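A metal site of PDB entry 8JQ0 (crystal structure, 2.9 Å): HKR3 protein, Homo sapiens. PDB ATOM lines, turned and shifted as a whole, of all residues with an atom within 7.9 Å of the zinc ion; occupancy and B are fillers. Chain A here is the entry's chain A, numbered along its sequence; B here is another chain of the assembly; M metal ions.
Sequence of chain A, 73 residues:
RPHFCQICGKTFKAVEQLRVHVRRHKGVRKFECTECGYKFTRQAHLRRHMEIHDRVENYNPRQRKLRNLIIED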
ATOM      1  N   GLU A  32      22.642  -2.896  33.112  1.00  0.00           N
ATOM      2  CA  GLU A  32      22.469  -2.468  31.729  1.00  0.00           C
ATOM      3  C   GLU A  32      22.845  -3.613  30.795  1.00  0.00           C
ATOM      4  O   GLU A  32      23.856  -4.293  30.998  1.00  0.00           O
ATOM      5  CB  GLU A  32      23.331  -1.237  31.430  1.00  0.00           C
ATOM      6  CG  GLU A  32      22.942  -0.490  30.177  1.00  0.00           C
ATOM      7  CD  GLU A  32      24.007   0.486  29.728  1.00  0.00           C
ATOM      8  OE1 GLU A  32      25.191   0.071  29.610  1.00  0.00           O
ATOM      9  OE2 GLU A  32      23.681   1.668  29.488  1.00  0.00           O
ATOM     10  N   CYS A  33      22.024  -3.807  29.763  1.00  0.00           N
ATOM     11  CA  CYS A  33      22.316  -4.826  28.765  1.00  0.00           C
ATOM     12  C   CYS A  33      23.475  -4.391  27.883  1.00  0.00           C
ATOM     13  O   CYS A  33      23.510  -3.256  27.404  1.00  0.00           O
ATOM     14  CB  CYS A  33      21.072  -5.113  27.916  1.00  0.00           C
ATOM     15  SG  CYS A  33      21.362  -6.249  26.538  1.00  0.00           S
ATOM     16  N   THR A  34      24.433  -5.294  27.676  1.00  0.00           N
ATOM     17  CA  THR A  34      25.630  -4.966  26.910  1.00  0.00           C
ATOM     18  C   THR A  34      25.426  -5.193  25.423  1.00  0.00           C
ATOM     19  O   THR A  34      26.391  -5.448  24.695  1.00  0.00           O
ATOM     20  CB  THR A  34      26.825  -5.792  27.413  1.00  0.00           C
ATOM     21  OG1 THR A  34      26.460  -7.171  27.509  1.00  0.00           O
ATOM     22  CG2 THR A  34      27.287  -5.287  28.772  1.00  0.00           C
ATOM     23  N   GLU A  35      24.184  -5.101  24.954  1.00  0.00           N
ATOM     24  CA  GLU A  35      23.891  -5.276  23.536  1.00  0.00           C
ATOM     25  C   GLU A  35      22.995  -4.158  23.027  1.00  0.00           C
ATOM     26  O   GLU A  35      23.298  -3.531  22.004  1.00  0.00           O
ATOM     27  CB  GLU A  35      23.247  -6.642  23.291  1.00  0.00           C
ATOM     28  CG  GLU A  35      24.219  -7.808  23.403  1.00  0.00           C
ATOM     29  CD  GLU A  35      23.742  -9.030  22.653  1.00  0.00           C
ATOM     30  OE1 GLU A  35      22.886  -8.884  21.752  1.00  0.00           O
ATOM     31  OE2 GLU A  35      24.212 -10.148  22.958  1.00  0.00           O
ATOM     32  N   CYS A  36      21.890  -3.893  23.724  1.00  0.00           N
ATOM     33  CA  CYS A  36      20.994  -2.815  23.360  1.00  0.00           C
ATOM     34  C   CYS A  36      21.019  -1.651  24.348  1.00  0.00           C
ATOM     35  O   CYS A  36      20.256  -0.695  24.179  1.00  0.00           O
ATOM     36  CB  CYS A  36      19.561  -3.348  23.223  1.00  0.00           C
ATOM     37  SG  CYS A  36      18.645  -3.503  24.776  1.00  0.00           S
ATOM     38  N   GLY A  37      21.879  -1.722  25.373  1.00  0.00           N
ATOM     39  CA  GLY A  37      22.058  -0.614  26.284  1.00  0.00           C
ATOM     40  C   GLY A  37      20.889  -0.303  27.192  1.00  0.00           C
ATOM     41  O   GLY A  37      20.864   0.767  27.809  1.00  0.00           O
ATOM     42  N   TYR A  38      19.914  -1.208  27.296  1.00  0.00           N
ATOM     43  CA  TYR A  38      18.739  -0.955  28.118  1.00  0.00           C
ATOM     44  C   TYR A  38      19.060  -1.201  29.591  1.00  0.00           C
ATOM     45  O   TYR A  38      19.682  -2.206  29.935  1.00  0.00           O
ATOM     46  CB  TYR A  38      17.582  -1.856  27.670  1.00  0.00           C
ATOM     47  CG  TYR A  38      16.299  -1.628  28.420  1.00  0.00           C
ATOM     48  CD1 TYR A  38      15.526  -2.696  28.846  1.00  0.00           C
ATOM     49  CD2 TYR A  38      15.849  -0.346  28.706  1.00  0.00           C
ATOM     50  CE1 TYR A  38      14.349  -2.502  29.527  1.00  0.00           C
ATOM     51  CE2 TYR A  38      14.668  -0.144  29.388  1.00  0.00           C
ATOM     52  CZ  TYR A  38      13.918  -1.221  29.798  1.00  0.00           C
ATOM     53  OH  TYR A  38      12.745  -1.015  30.485  1.00  0.00           O
ATOM     54  N   LYS A  39      18.638  -0.273  30.443  1.00  0.00           N
ATOM     55  CA  LYS A  39      18.931  -0.339  31.869  1.00  0.00           C
ATOM     56  C   LYS A  39      17.816  -1.046  32.622  1.00  0.00           C
ATOM     57  O   LYS A  39      16.636  -0.890  32.286  1.00  0.00           O
ATOM     58  CB  LYS A  39      19.151   1.069  32.437  1.00  0.00           C
ATOM     59  CG  LYS A  39      20.420   1.732  31.944  1.00  0.00           C
ATOM     60  CD  LYS A  39      20.511   3.187  32.408  1.00  0.00           C
ATOM     61  CE  LYS A  39      21.425   3.994  31.492  1.00  0.00           C
ATOM     62  NZ  LYS A  39      20.686   5.052  30.760  1.00  0.00           N
ATOM     63  N   PHE A  40      18.194  -1.823  33.638  1.00  0.00           N
ATOM     64  CA  PHE A  40      17.269  -2.656  34.386  1.00  0.00           C
ATOM     65  C   PHE A  40      17.355  -2.358  35.869  1.00  0.00           C
ATOM     66  O   PHE A  40      18.400  -1.915  36.372  1.00  0.00           O
ATOM     67  CB  PHE A  40      17.547  -4.148  34.148  1.00  0.00           C
ATOM     68  CG  PHE A  40      17.082  -4.646  32.812  1.00  0.00           C
ATOM     69  CD1 PHE A  40      15.730  -4.756  32.541  1.00  0.00           C
ATOM     70  CD2 PHE A  40      17.993  -4.992  31.835  1.00  0.00           C
ATOM     71  CE1 PHE A  40      15.305  -5.218  31.310  1.00  0.00           C
ATOM     72  CE2 PHE A  40      17.565  -5.456  30.612  1.00  0.00           C
ATOM     73  CZ  PHE A  40      16.221  -5.563  30.346  1.00  0.00           C
ATOM     74  N   LEU A  46      17.518  -8.622  33.748  1.00  0.00           N
ATOM     75  CA  LEU A  46      18.520  -8.580  32.687  1.00  0.00           C
ATOM     76  C   LEU A  46      18.744  -9.961  32.081  1.00  0.00           C
ATOM     77  O   LEU A  46      18.800 -10.100  30.857  1.00  0.00           O
ATOM     78  CB  LEU A  46      19.837  -8.018  33.244  1.00  0.00           C
ATOM     79  CG  LEU A  46      20.997  -7.748  32.291  1.00  0.00           C
ATOM     80  CD1 LEU A  46      20.506  -7.302  30.920  1.00  0.00           C
ATOM     81  CD2 LEU A  46      21.957  -6.720  32.898  1.00  0.00           C
ATOM     82  N   HIS A  49      16.029 -10.937  29.952  1.00  0.00           N
ATOM     83  CA  HIS A  49      15.986 -10.146  28.728  1.00  0.00           C
ATOM     84  C   HIS A  49      16.886 -10.733  27.642  1.00  0.00           C
ATOM     85  O   HIS A  49      16.550 -10.682  26.451  1.00  0.00           O
ATOM     86  CB  HIS A  49      16.395  -8.701  29.036  1.00  0.00           C
ATOM     87  CG  HIS A  49      16.722  -7.887  27.832  1.00  0.00           C
ATOM     88  ND1 HIS A  49      15.763  -7.227  27.096  1.00  0.00           N
ATOM     89  CD2 HIS A  49      17.909  -7.607  27.238  1.00  0.00           C
ATOM     90  CE1 HIS A  49      16.342  -6.585  26.099  1.00  0.00           C
ATOM     91  NE2 HIS A  49      17.643  -6.798  26.165  1.00  0.00           N
ATOM     92  N   MET A  50      18.034 -11.304  28.033  1.00  0.00           N
ATOM     93  CA  MET A  50      18.922 -11.885  27.033  1.00  0.00           C
ATOM     94  C   MET A  50      18.371 -13.166  26.426  1.00  0.00           C
ATOM     95  O   MET A  50      18.800 -13.560  25.343  1.00  0.00           O
ATOM     96  CB  MET A  50      20.301 -12.176  27.632  1.00  0.00           C
ATOM     97  CG  MET A  50      21.444 -11.524  26.884  1.00  0.00           C
ATOM     98  SD  MET A  50      21.679  -9.802  27.362  1.00  0.00           S
ATOM     99  CE  MET A  50      21.946 -10.010  29.126  1.00  0.00           C
ATOM    100  N   HIS A  53      17.141 -12.097  23.347  1.00  0.00           N
ATOM    101  CA  HIS A  53      18.194 -11.722  22.416  1.00  0.00           C
ATOM    102  C   HIS A  53      18.722 -12.920  21.638  1.00  0.00           C
ATOM    103  O   HIS A  53      19.334 -12.748  20.582  1.00  0.00           O
ATOM    104  CB  HIS A  53      19.346 -11.035  23.166  1.00  0.00           C
ATOM    105  CG  HIS A  53      19.242  -9.542  23.195  1.00  0.00           C
ATOM    106  ND1 HIS A  53      18.976  -8.792  22.071  1.00  0.00           N
ATOM    107  CD2 HIS A  53      19.379  -8.662  24.212  1.00  0.00           C
ATOM    108  CE1 HIS A  53      18.953  -7.509  22.394  1.00  0.00           C
ATOM    109  NE2 HIS A  53      19.192  -7.408  23.691  1.00  0.00           N
ATOM    110  N   TYR A  59      16.940  -6.729  18.114  1.00  0.00           N
ATOM    111  CA  TYR A  59      16.110  -6.405  19.273  1.00  0.00           C
ATOM    112  C   TYR A  59      16.594  -5.070  19.836  1.00  0.00           C
ATOM    113  O   TYR A  59      17.764  -4.938  20.197  1.00  0.00           O
ATOM    114  CB  TYR A  59      16.211  -7.502  20.342  1.00  0.00           C
ATOM    115  CG  TYR A  59      15.076  -7.496  21.353  1.00  0.00           C
ATOM    116  CD1 TYR A  59      14.726  -8.657  22.032  1.00  0.00           C
ATOM    117  CD2 TYR A  59      14.338  -6.353  21.606  1.00  0.00           C
ATOM    118  CE1 TYR A  59      13.687  -8.653  22.947  1.00  0.00           C
ATOM    119  CE2 TYR A  59      13.303  -6.346  22.512  1.00  0.00           C
ATOM    120  CZ  TYR A  59      12.981  -7.505  23.181  1.00  0.00           C
ATOM    121  OH  TYR A  59      11.941  -7.522  24.089  1.00  0.00           O
ATOM    122  N   ASN A  60      15.680  -4.102  19.935  1.00  0.00           N
ATOM    123  CA  ASN A  60      15.988  -2.830  20.588  1.00  0.00           C
ATOM    124  C   ASN A  60      14.703  -2.194  21.121  1.00  0.00           C
ATOM    125  O   ASN A  60      13.975  -1.541  20.353  1.00  0.00           O
ATOM    126  CB  ASN A  60      16.693  -1.887  19.617  1.00  0.00           C
ATOM    127  CG  ASN A  60      17.831  -1.117  20.264  1.00  0.00           C
ATOM    128  OD1 ASN A  60      17.616  -0.099  20.923  1.00  0.00           O
ATOM    129  ND2 ASN A  60      19.054  -1.592  20.065  1.00  0.00           N
ATOM    130  N   PRO A  61      14.409  -2.338  22.412  1.00  0.00           N
ATOM    131  CA  PRO A  61      13.168  -1.759  22.946  1.00  0.00           C
ATOM    132  C   PRO A  61      13.391  -0.338  23.430  1.00  0.00           C
ATOM    133  O   PRO A  61      14.501   0.081  23.729  1.00  0.00           O
ATOM    134  CB  PRO A  61      12.831  -2.675  24.150  1.00  0.00           C
ATOM    135  CG  PRO A  61      13.988  -3.585  24.322  1.00  0.00           C
ATOM    136  CD  PRO A  61      15.069  -3.258  23.343  1.00  0.00           C
ATOM    137  P    DA B   9      12.158  -7.221  28.249  1.00  0.00           P
ATOM    138  OP1  DA B   9      13.041  -6.786  27.144  1.00  0.00           O
ATOM    139  OP2  DA B   9      12.389  -8.528  28.905  1.00  0.00           O
ATOM    140  O5'  DA B   9      12.162  -6.093  29.374  1.00  0.00           O
ATOM    141  C5'  DA B   9      11.820  -4.764  29.037  1.00  0.00           C
ATOM    142  C4'  DA B   9      10.889  -4.150  30.073  1.00  0.00           C
ATOM    143  O4'  DA B   9       9.709  -4.993  30.214  1.00  0.00           O
ATOM    144  C3'  DA B   9      11.483  -3.999  31.470  1.00  0.00           C
ATOM    145  O3'  DA B   9      11.109  -2.727  32.007  1.00  0.00           O
ATOM    146  C2'  DA B   9      10.832  -5.146  32.246  1.00  0.00           C
ATOM    147  C1'  DA B   9       9.475  -5.241  31.577  1.00  0.00           C
ATOM    148  N9   DA B   9       8.847  -6.548  31.701  1.00  0.00           N
ATOM    149  C8   DA B   9       9.334  -7.740  31.255  1.00  0.00           C
ATOM    150  N7   DA B   9       8.551  -8.769  31.510  1.00  0.00           N
ATOM    151  C5   DA B   9       7.469  -8.194  32.174  1.00  0.00           C
ATOM    152  C6   DA B   9       6.290  -8.748  32.713  1.00  0.00           C
ATOM    153  N6   DA B   9       5.998 -10.055  32.659  1.00  0.00           N
ATOM    154  N1   DA B   9       5.421  -7.910  33.304  1.00  0.00           N
ATOM    155  C2   DA B   9       5.717  -6.600  33.349  1.00  0.00           C
ATOM    156  N3   DA B   9       6.795  -5.967  32.883  1.00  0.00           N
ATOM    157  C4   DA B   9       7.635  -6.828  32.296  1.00  0.00           C
HETATM  158 ZN    ZN M   1      19.330  -5.670  25.283  1.00  0.00          ZN
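Along chain A the residues within 4 Å of the zinc ion span positions 33 to 53. The nearest printed residue that does not touch the zinc ion is Glu 35 (4.5 Å).
The zinc ion is bound by NE2 of His 49, SG of Cys 36, NE2 of His 53 and SG of Cys 33. The zinc ion has four donor atoms within binding distance.
The side-chain sulfur (SG) of Cys 33 lies close to the backbone NH (N) of Glu 35, 3.4 Å away. The backbone NH of Tyr 38 lies close to the side-chain sulfur of Cys 36 (3.6 Å). A ring nitrogen (ND1) of His 49 lies within hydrogen-bond range of OP1 of DA 9 of chain B (2.8 Å). SD of Met 50 sits close to SG of Cys 33 (3.7 Å). The backbone carbonyl oxygen of Tyr 38 sits at hydrogen-bond distance from the backbone NH of Cys 33 (2.8 Å).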
